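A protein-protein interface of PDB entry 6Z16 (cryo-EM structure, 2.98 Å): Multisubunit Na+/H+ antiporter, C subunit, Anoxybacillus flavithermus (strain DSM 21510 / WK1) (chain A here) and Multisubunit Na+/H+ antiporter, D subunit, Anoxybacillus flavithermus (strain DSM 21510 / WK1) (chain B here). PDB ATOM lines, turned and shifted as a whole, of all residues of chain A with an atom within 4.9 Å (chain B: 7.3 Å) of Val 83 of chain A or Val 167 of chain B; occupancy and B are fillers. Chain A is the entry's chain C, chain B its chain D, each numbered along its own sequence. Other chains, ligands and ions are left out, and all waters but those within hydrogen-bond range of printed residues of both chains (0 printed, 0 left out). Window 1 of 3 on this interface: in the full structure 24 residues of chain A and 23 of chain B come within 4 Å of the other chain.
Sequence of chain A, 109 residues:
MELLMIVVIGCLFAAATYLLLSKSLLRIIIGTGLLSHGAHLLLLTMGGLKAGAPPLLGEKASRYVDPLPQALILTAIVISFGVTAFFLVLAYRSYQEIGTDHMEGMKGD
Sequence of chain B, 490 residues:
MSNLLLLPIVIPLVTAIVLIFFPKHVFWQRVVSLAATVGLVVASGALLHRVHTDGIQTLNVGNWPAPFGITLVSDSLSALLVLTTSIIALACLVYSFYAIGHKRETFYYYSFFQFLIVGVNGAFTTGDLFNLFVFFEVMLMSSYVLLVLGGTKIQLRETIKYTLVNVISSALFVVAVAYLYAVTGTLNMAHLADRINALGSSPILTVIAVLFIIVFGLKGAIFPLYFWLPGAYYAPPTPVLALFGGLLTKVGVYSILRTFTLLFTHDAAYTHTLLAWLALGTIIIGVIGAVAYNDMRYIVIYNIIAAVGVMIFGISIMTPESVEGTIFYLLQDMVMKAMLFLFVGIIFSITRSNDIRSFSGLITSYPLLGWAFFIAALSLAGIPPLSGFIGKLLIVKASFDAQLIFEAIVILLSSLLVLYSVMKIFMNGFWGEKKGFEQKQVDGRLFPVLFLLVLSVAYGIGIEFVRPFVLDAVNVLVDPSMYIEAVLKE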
ATOM      1  N   THR A  32     -16.494 -16.489  15.869  1.00  0.00           N
ATOM      2  CA  THR A  32     -16.116 -17.336  14.738  1.00  0.00           C
ATOM      3  C   THR A  32     -14.972 -18.278  15.104  1.00  0.00           C
ATOM      4  O   THR A  32     -15.024 -19.485  14.816  1.00  0.00           O
ATOM      5  CB  THR A  32     -15.736 -16.449  13.550  1.00  0.00           C
ATOM      6  OG1 THR A  32     -16.912 -15.856  12.984  1.00  0.00           O
ATOM      7  CG2 THR A  32     -14.944 -17.204  12.503  1.00  0.00           C
ATOM      8  N   ILE A  79      -8.273 -24.396   6.169  1.00  0.00           N
ATOM      9  CA  ILE A  79      -9.344 -23.658   5.498  1.00  0.00           C
ATOM     10  C   ILE A  79      -9.897 -22.552   6.401  1.00  0.00           C
ATOM     11  O   ILE A  79     -10.080 -21.401   5.966  1.00  0.00           O
ATOM     12  CB  ILE A  79     -10.445 -24.629   5.040  1.00  0.00           C
ATOM     13  CG1 ILE A  79      -9.937 -25.499   3.896  1.00  0.00           C
ATOM     14  CG2 ILE A  79     -11.684 -23.894   4.619  1.00  0.00           C
ATOM     15  CD1 ILE A  79     -10.849 -26.635   3.545  1.00  0.00           C
ATOM     16  N   SER A  80     -10.141 -22.880   7.676  1.00  0.00           N
ATOM     17  CA  SER A  80     -10.634 -21.905   8.640  1.00  0.00           C
ATOM     18  C   SER A  80      -9.639 -20.784   8.869  1.00  0.00           C
ATOM     19  O   SER A  80     -10.045 -19.637   9.059  1.00  0.00           O
ATOM     20  CB  SER A  80     -10.954 -22.597   9.963  1.00  0.00           C
ATOM     21  OG  SER A  80     -11.986 -23.548   9.802  1.00  0.00           O
ATOM     22  N   PHE A  81      -8.339 -21.088   8.827  1.00  0.00           N
ATOM     23  CA  PHE A  81      -7.337 -20.037   8.963  1.00  0.00           C
ATOM     24  C   PHE A  81      -7.343 -19.093   7.773  1.00  0.00           C
ATOM     25  O   PHE A  81      -7.191 -17.877   7.949  1.00  0.00           O
ATOM     26  CB  PHE A  81      -5.944 -20.630   9.150  1.00  0.00           C
ATOM     27  CG  PHE A  81      -4.858 -19.597   9.120  1.00  0.00           C
ATOM     28  CD1 PHE A  81      -4.755 -18.655  10.129  1.00  0.00           C
ATOM     29  CD2 PHE A  81      -3.952 -19.558   8.072  1.00  0.00           C
ATOM     30  CE1 PHE A  81      -3.774 -17.693  10.096  1.00  0.00           C
ATOM     31  CE2 PHE A  81      -2.964 -18.601   8.038  1.00  0.00           C
ATOM     32  CZ  PHE A  81      -2.875 -17.667   9.050  1.00  0.00           C
ATOM     33  N   GLY A  82      -7.505 -19.634   6.558  1.00  0.00           N
ATOM     34  CA  GLY A  82      -7.595 -18.772   5.384  1.00  0.00           C
ATOM     35  C   GLY A  82      -8.779 -17.824   5.439  1.00  0.00           C
ATOM     36  O   GLY A  82      -8.637 -16.608   5.230  1.00  0.00           O
ATOM     37  N   VAL A  83      -9.954 -18.360   5.784  1.00  0.00           N
ATOM     38  CA  VAL A  83     -11.156 -17.529   5.848  1.00  0.00           C
ATOM     39  C   VAL A  83     -11.072 -16.532   7.007  1.00  0.00           C
ATOM     40  O   VAL A  83     -11.496 -15.377   6.881  1.00  0.00           O
ATOM     41  CB  VAL A  83     -12.408 -18.420   5.941  1.00  0.00           C
ATOM     42  CG1 VAL A  83     -13.657 -17.584   5.936  1.00  0.00           C
ATOM     43  CG2 VAL A  83     -12.442 -19.410   4.790  1.00  0.00           C
ATOM     44  N   THR A  84     -10.461 -16.939   8.125  1.00  0.00           N
ATOM     45  CA  THR A  84     -10.332 -16.065   9.286  1.00  0.00           C
ATOM     46  C   THR A  84      -9.383 -14.905   9.012  1.00  0.00           C
ATOM     47  O   THR A  84      -9.664 -13.764   9.402  1.00  0.00           O
ATOM     48  CB  THR A  84      -9.847 -16.883  10.484  1.00  0.00           C
ATOM     49  OG1 THR A  84     -10.745 -17.974  10.710  1.00  0.00           O
ATOM     50  CG2 THR A  84      -9.802 -16.033  11.737  1.00  0.00           C
ATOM     51  N   ALA A  85      -8.268 -15.173   8.327  1.00  0.00           N
ATOM     52  CA  ALA A  85      -7.336 -14.111   7.974  1.00  0.00           C
ATOM     53  C   ALA A  85      -7.961 -13.128   6.996  1.00  0.00           C
ATOM     54  O   ALA A  85      -7.789 -11.906   7.140  1.00  0.00           O
ATOM     55  CB  ALA A  85      -6.064 -14.712   7.382  1.00  0.00           C
ATOM     56  N   PHE A  86      -8.710 -13.649   6.013  1.00  0.00           N
ATOM     57  CA  PHE A  86      -9.434 -12.784   5.084  1.00  0.00           C
ATOM     58  C   PHE A  86     -10.450 -11.901   5.800  1.00  0.00           C
ATOM     59  O   PHE A  86     -10.530 -10.695   5.536  1.00  0.00           O
ATOM     60  CB  PHE A  86     -10.127 -13.633   4.022  1.00  0.00           C
ATOM     61  CG  PHE A  86     -11.019 -12.845   3.109  1.00  0.00           C
ATOM     62  CD1 PHE A  86     -10.484 -12.020   2.136  1.00  0.00           C
ATOM     63  CD2 PHE A  86     -12.398 -12.934   3.226  1.00  0.00           C
ATOM     64  CE1 PHE A  86     -11.309 -11.293   1.301  1.00  0.00           C
ATOM     65  CE2 PHE A  86     -13.222 -12.205   2.403  1.00  0.00           C
ATOM     66  CZ  PHE A  86     -12.679 -11.385   1.439  1.00  0.00           C
ATOM     67  N   PHE A  87     -11.205 -12.478   6.734  1.00  0.00           N
ATOM     68  CA  PHE A  87     -12.265 -11.737   7.405  1.00  0.00           C
ATOM     69  C   PHE A  87     -11.701 -10.723   8.394  1.00  0.00           C
ATOM     70  O   PHE A  87     -12.287  -9.652   8.581  1.00  0.00           O
ATOM     71  CB  PHE A  87     -13.216 -12.754   8.042  1.00  0.00           C
ATOM     72  CG  PHE A  87     -14.466 -12.171   8.616  1.00  0.00           C
ATOM     73  CD1 PHE A  87     -15.260 -11.319   7.869  1.00  0.00           C
ATOM     74  CD2 PHE A  87     -14.935 -12.610   9.836  1.00  0.00           C
ATOM     75  CE1 PHE A  87     -16.437 -10.811   8.389  1.00  0.00           C
ATOM     76  CE2 PHE A  87     -16.120 -12.126  10.352  1.00  0.00           C
ATOM     77  CZ  PHE A  87     -16.870 -11.223   9.626  1.00  0.00           C
ATOM     78  N   GLU B 137     -15.943 -24.637  -0.016  1.00  0.00           N
ATOM     79  CA  GLU B 137     -15.132 -23.497   0.414  1.00  0.00           C
ATOM     80  C   GLU B 137     -14.288 -22.884  -0.690  1.00  0.00           C
ATOM     81  O   GLU B 137     -13.996 -21.689  -0.610  1.00  0.00           O
ATOM     82  CB  GLU B 137     -14.232 -23.813   1.604  1.00  0.00           C
ATOM     83  CG  GLU B 137     -14.943 -23.524   2.898  1.00  0.00           C
ATOM     84  CD  GLU B 137     -15.560 -24.730   3.481  1.00  0.00           C
ATOM     85  OE1 GLU B 137     -15.073 -25.819   3.167  1.00  0.00           O
ATOM     86  OE2 GLU B 137     -16.567 -24.594   4.192  1.00  0.00           O
ATOM     87  N   LEU B 140     -16.976 -20.665  -2.198  1.00  0.00           N
ATOM     88  CA  LEU B 140     -17.358 -19.574  -1.310  1.00  0.00           C
ATOM     89  C   LEU B 140     -16.232 -18.574  -1.118  1.00  0.00           C
ATOM     90  O   LEU B 140     -16.491 -17.374  -1.019  1.00  0.00           O
ATOM     91  CB  LEU B 140     -17.821 -20.114   0.039  1.00  0.00           C
ATOM     92  CG  LEU B 140     -19.218 -20.726   0.093  1.00  0.00           C
ATOM     93  CD1 LEU B 140     -19.453 -21.350   1.450  1.00  0.00           C
ATOM     94  CD2 LEU B 140     -20.255 -19.666  -0.204  1.00  0.00           C
ATOM     95  N   MET B 141     -14.980 -19.033  -1.084  1.00  0.00           N
ATOM     96  CA  MET B 141     -13.858 -18.117  -0.932  1.00  0.00           C
ATOM     97  C   MET B 141     -13.709 -17.224  -2.156  1.00  0.00           C
ATOM     98  O   MET B 141     -13.541 -15.995  -2.027  1.00  0.00           O
ATOM     99  CB  MET B 141     -12.584 -18.916  -0.677  1.00  0.00           C
ATOM    100  CG  MET B 141     -11.427 -18.068  -0.246  1.00  0.00           C
ATOM    101  SD  MET B 141     -11.725 -17.372   1.377  1.00  0.00           S
ATOM    102  CE  MET B 141     -10.833 -15.848   1.197  1.00  0.00           C
ATOM    103  N   TYR B 144     -16.471 -14.658  -2.005  1.00  0.00           N
ATOM    104  CA  TYR B 144     -16.123 -13.584  -1.067  1.00  0.00           C
ATOM    105  C   TYR B 144     -15.267 -12.533  -1.745  1.00  0.00           C
ATOM    106  O   TYR B 144     -15.519 -11.325  -1.627  1.00  0.00           O
ATOM    107  CB  TYR B 144     -15.315 -14.107   0.121  1.00  0.00           C
ATOM    108  CG  TYR B 144     -15.917 -15.124   1.043  1.00  0.00           C
ATOM    109  CD1 TYR B 144     -17.285 -15.292   1.179  1.00  0.00           C
ATOM    110  CD2 TYR B 144     -15.081 -15.955   1.764  1.00  0.00           C
ATOM    111  CE1 TYR B 144     -17.790 -16.268   2.027  1.00  0.00           C
ATOM    112  CE2 TYR B 144     -15.567 -16.913   2.595  1.00  0.00           C
ATOM    113  CZ  TYR B 144     -16.911 -17.070   2.728  1.00  0.00           C
ATOM    114  OH  TYR B 144     -17.336 -18.049   3.581  1.00  0.00           O
ATOM    115  N   LYS B 161     -21.365  -9.166   5.920  1.00  0.00           N
ATOM    116  CA  LYS B 161     -22.589  -9.934   6.185  1.00  0.00           C
ATOM    117  C   LYS B 161     -22.534 -11.335   5.562  1.00  0.00           C
ATOM    118  O   LYS B 161     -22.766 -12.351   6.244  1.00  0.00           O
ATOM    119  CB  LYS B 161     -23.803  -9.184   5.641  1.00  0.00           C
ATOM    120  CG  LYS B 161     -24.513  -8.186   6.557  1.00  0.00           C
ATOM    121  CD  LYS B 161     -23.667  -6.972   6.884  1.00  0.00           C
ATOM    122  CE  LYS B 161     -24.447  -5.916   7.641  1.00  0.00           C
ATOM    123  NZ  LYS B 161     -25.535  -5.348   6.818  1.00  0.00           N
ATOM    124  N   TYR B 162     -22.221 -11.396   4.260  1.00  0.00           N
ATOM    125  CA  TYR B 162     -22.190 -12.649   3.510  1.00  0.00           C
ATOM    126  C   TYR B 162     -21.136 -13.609   4.055  1.00  0.00           C
ATOM    127  O   TYR B 162     -21.387 -14.821   4.185  1.00  0.00           O
ATOM    128  CB  TYR B 162     -21.934 -12.309   2.040  1.00  0.00           C
ATOM    129  CG  TYR B 162     -21.830 -13.461   1.082  1.00  0.00           C
ATOM    130  CD1 TYR B 162     -22.948 -14.182   0.712  1.00  0.00           C
ATOM    131  CD2 TYR B 162     -20.618 -13.791   0.500  1.00  0.00           C
ATOM    132  CE1 TYR B 162     -22.858 -15.225  -0.183  1.00  0.00           C
ATOM    133  CE2 TYR B 162     -20.518 -14.830  -0.394  1.00  0.00           C
ATOM    134  CZ  TYR B 162     -21.643 -15.545  -0.730  1.00  0.00           C
ATOM    135  OH  TYR B 162     -21.554 -16.584  -1.618  1.00  0.00           O
ATOM    136  N   THR B 163     -19.970 -13.069   4.431  1.00  0.00           N
ATOM    137  CA  THR B 163     -18.881 -13.882   4.954  1.00  0.00           C
ATOM    138  C   THR B 163     -19.247 -14.478   6.301  1.00  0.00           C
ATOM    139  O   THR B 163     -18.972 -15.658   6.553  1.00  0.00           O
ATOM    140  CB  THR B 163     -17.621 -13.030   5.079  1.00  0.00           C
ATOM    141  OG1 THR B 163     -17.386 -12.349   3.844  1.00  0.00           O
ATOM    142  CG2 THR B 163     -16.429 -13.904   5.375  1.00  0.00           C
ATOM    143  N   LEU B 164     -19.900 -13.679   7.155  1.00  0.00           N
ATOM    144  CA  LEU B 164     -20.341 -14.136   8.469  1.00  0.00           C
ATOM    145  C   LEU B 164     -21.296 -15.325   8.354  1.00  0.00           C
ATOM    146  O   LEU B 164     -21.116 -16.356   9.030  1.00  0.00           O
ATOM    147  CB  LEU B 164     -21.008 -12.957   9.174  1.00  0.00           C
ATOM    148  CG  LEU B 164     -21.209 -12.789  10.674  1.00  0.00           C
ATOM    149  CD1 LEU B 164     -21.364 -11.304  10.924  1.00  0.00           C
ATOM    150  CD2 LEU B 164     -22.406 -13.531  11.174  1.00  0.00           C
ATOM    151  N   VAL B 165     -22.284 -15.208   7.453  1.00  0.00           N
ATOM    152  CA  VAL B 165     -23.272 -16.276   7.272  1.00  0.00           C
ATOM    153  C   VAL B 165     -22.617 -17.553   6.761  1.00  0.00           C
ATOM    154  O   VAL B 165     -22.906 -18.660   7.247  1.00  0.00           O
ATOM    155  CB  VAL B 165     -24.387 -15.816   6.317  1.00  0.00           C
ATOM    156  CG1 VAL B 165     -25.404 -16.924   6.101  1.00  0.00           C
ATOM    157  CG2 VAL B 165     -25.053 -14.623   6.861  1.00  0.00           C
ATOM    158  N   ASN B 166     -21.704 -17.423   5.798  1.00  0.00           N
ATOM    159  CA  ASN B 166     -21.134 -18.631   5.214  1.00  0.00           C
ATOM    160  C   ASN B 166     -20.125 -19.301   6.137  1.00  0.00           C
ATOM    161  O   ASN B 166     -19.955 -20.522   6.067  1.00  0.00           O
ATOM    162  CB  ASN B 166     -20.515 -18.306   3.870  1.00  0.00           C
ATOM    163  CG  ASN B 166     -21.543 -17.968   2.842  1.00  0.00           C
ATOM    164  OD1 ASN B 166     -22.547 -18.663   2.698  1.00  0.00           O
ATOM    165  ND2 ASN B 166     -21.326 -16.875   2.142  1.00  0.00           N
ATOM    166  N   VAL B 167     -19.480 -18.536   7.026  1.00  0.00           N
ATOM    167  CA  VAL B 167     -18.625 -19.137   8.051  1.00  0.00           C
ATOM    168  C   VAL B 167     -19.453 -19.990   9.006  1.00  0.00           C
ATOM    169  O   VAL B 167     -19.082 -21.133   9.331  1.00  0.00           O
ATOM    170  CB  VAL B 167     -17.846 -18.047   8.807  1.00  0.00           C
ATOM    171  CG1 VAL B 167     -17.235 -18.612  10.041  1.00  0.00           C
ATOM    172  CG2 VAL B 167     -16.741 -17.509   7.950  1.00  0.00           C
ATOM    173  N   ILE B 168     -20.598 -19.451   9.447  1.00  0.00           N
ATOM    174  CA  ILE B 168     -21.480 -20.207  10.340  1.00  0.00           C
ATOM    175  C   ILE B 168     -21.983 -21.486   9.672  1.00  0.00           C
ATOM    176  O   ILE B 168     -21.948 -22.573  10.271  1.00  0.00           O
ATOM    177  CB  ILE B 168     -22.633 -19.307  10.816  1.00  0.00           C
ATOM    178  CG1 ILE B 168     -22.079 -18.181  11.678  1.00  0.00           C
ATOM    179  CG2 ILE B 168     -23.664 -20.097  11.581  1.00  0.00           C
ATOM    180  CD1 ILE B 168     -23.078 -17.128  11.988  1.00  0.00           C
ATOM    181  N   SER B 169     -22.382 -21.396   8.401  1.00  0.00           N
ATOM    182  CA  SER B 169     -22.879 -22.583   7.707  1.00  0.00           C
ATOM    183  C   SER B 169     -21.769 -23.591   7.401  1.00  0.00           C
ATOM    184  O   SER B 169     -22.026 -24.802   7.362  1.00  0.00           O
ATOM    185  CB  SER B 169     -23.597 -22.168   6.429  1.00  0.00           C
ATOM    186  OG  SER B 169     -22.706 -21.539   5.530  1.00  0.00           O
ATOM    187  N   SER B 170     -20.532 -23.122   7.218  1.00  0.00           N
ATOM    188  CA  SER B 170     -19.406 -24.034   7.028  1.00  0.00           C
ATOM    189  C   SER B 170     -19.117 -24.836   8.289  1.00  0.00           C
ATOM    190  O   SER B 170     -18.869 -26.051   8.220  1.00  0.00           O
ATOM    191  CB  SER B 170     -18.177 -23.238   6.612  1.00  0.00           C
ATOM    192  OG  SER B 170     -18.391 -22.614   5.360  1.00  0.00           O
ATOM    193  N   ALA B 171     -19.148 -24.168   9.448  1.00  0.00           N
ATOM    194  CA  ALA B 171     -18.978 -24.875  10.716  1.00  0.00           C
ATOM    195  C   ALA B 171     -20.102 -25.879  10.951  1.00  0.00           C
ATOM    196  O   ALA B 171     -19.870 -26.977  11.481  1.00  0.00           O
ATOM    197  CB  ALA B 171     -18.901 -23.873  11.863  1.00  0.00           C
ATOM    198  N   LEU B 172     -21.324 -25.530  10.538  1.00  0.00           N
ATOM    199  CA  LEU B 172     -22.436 -26.467  10.670  1.00  0.00           C
ATOM    200  C   LEU B 172     -22.288 -27.672   9.746  1.00  0.00           C
ATOM    201  O   LEU B 172     -22.690 -28.785  10.113  1.00  0.00           O
ATOM    202  CB  LEU B 172     -23.754 -25.742  10.417  1.00  0.00           C
ATOM    203  CG  LEU B 172     -24.130 -24.728  11.501  1.00  0.00           C
ATOM    204  CD1 LEU B 172     -25.310 -23.885  11.081  1.00  0.00           C
ATOM    205  CD2 LEU B 172     -24.433 -25.447  12.801  1.00  0.00           C
ATOM    206  N   PHE B 173     -21.695 -27.493   8.562  1.00  0.00           N
ATOM    207  CA  PHE B 173     -21.468 -28.665   7.719  1.00  0.00           C
ATOM    208  C   PHE B 173     -20.365 -29.546   8.291  1.00  0.00           C
ATOM    209  O   PHE B 173     -20.425 -30.776   8.150  1.00  0.00           O
ATOM    210  CB  PHE B 173     -21.140 -28.267   6.280  1.00  0.00           C
ATOM    211  CG  PHE B 173     -21.156 -29.427   5.329  1.00  0.00           C
ATOM    212  CD1 PHE B 173     -22.353 -30.037   5.006  1.00  0.00           C
ATOM    213  CD2 PHE B 173     -19.997 -29.913   4.767  1.00  0.00           C
ATOM    214  CE1 PHE B 173     -22.391 -31.110   4.140  1.00  0.00           C
ATOM    215  CE2 PHE B 173     -20.034 -30.988   3.899  1.00  0.00           C
ATOM    216  CZ  PHE B 173     -21.229 -31.582   3.586  1.00  0.00           C
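OE2 of Glu 137 of chain B sits at hydrogen-bond distance from OG of Ser 170 of chain B (2.9 Å).
Among the printed residues, merely in contact across the chains: Phe 86 of chain A with Met 141 of chain B (3.6 Å), Phe 86 of chain A with Tyr 144 of chain B (3.6 Å), Thr 32 of chain A with Val 167 of chain B (3.6 Å), Val 83 of chain A with Val 167 of chain B (3.7 Å), Ile 79 of chain A with Glu 137 of chain B (3.7 Å), Phe 87 of chain A with Thr 163 of chain B (3.8 Å) and Val 83 of chain A with Tyr 144 of chain B (3.9 Å).
Printed residues of chain B within 4 Å of Thr 32 of chain A: Val 167 (3.6 Å). Val 83 of chain A touches just these residues of chain B: Tyr 144 and Val 167. Printed residues of chain B within 4 Å of Phe 87 of chain A: Thr 163 (3.8 Å). Printed residues of chain A within 4 Å of Thr 163 of chain B: Phe 87. Of chain A, only Thr 32 (3.6 Å) and Val 83 (3.7 Å) come within 4 Å of Val 167 of chain B. The nearest residue of chain B that does not touch Val 83 of chain A is Met 141 of chain B (4.04 Å). The nearest printed residue of chain A that does not touch Val 167 of chain B is Phe 87 of chain A (5.6 Å).
Of the 17 printed residues of chain B, 5 touch a printed residue of chain A. Printed residues of chain B that touch a printed residue of chain A: Glu 137, Met 141, Tyr 144, Thr 163 and Val 167. Hydrophobic or aromatic side chains of chain B within 4 Å of the printed part of chain A: Met 141, Tyr 144 and Val 167. Along chain B the printed residues that touch a printed residue of chain A span positions 137 to 167. Of the 10 printed residues of chain A, 5 touch a printed residue of chain B. Hydrophobic or aromatic side chains of chain A that line the printed part of chain B: Ile 79, Val 83, Phe 86 and Phe 87. Among the printed residues, 7 pairs touch across the chains. Among the printed residues, no Asp or Glu carboxylate lies within 4 Å of a Lys or Arg side-chain nitrogen of the other chain.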
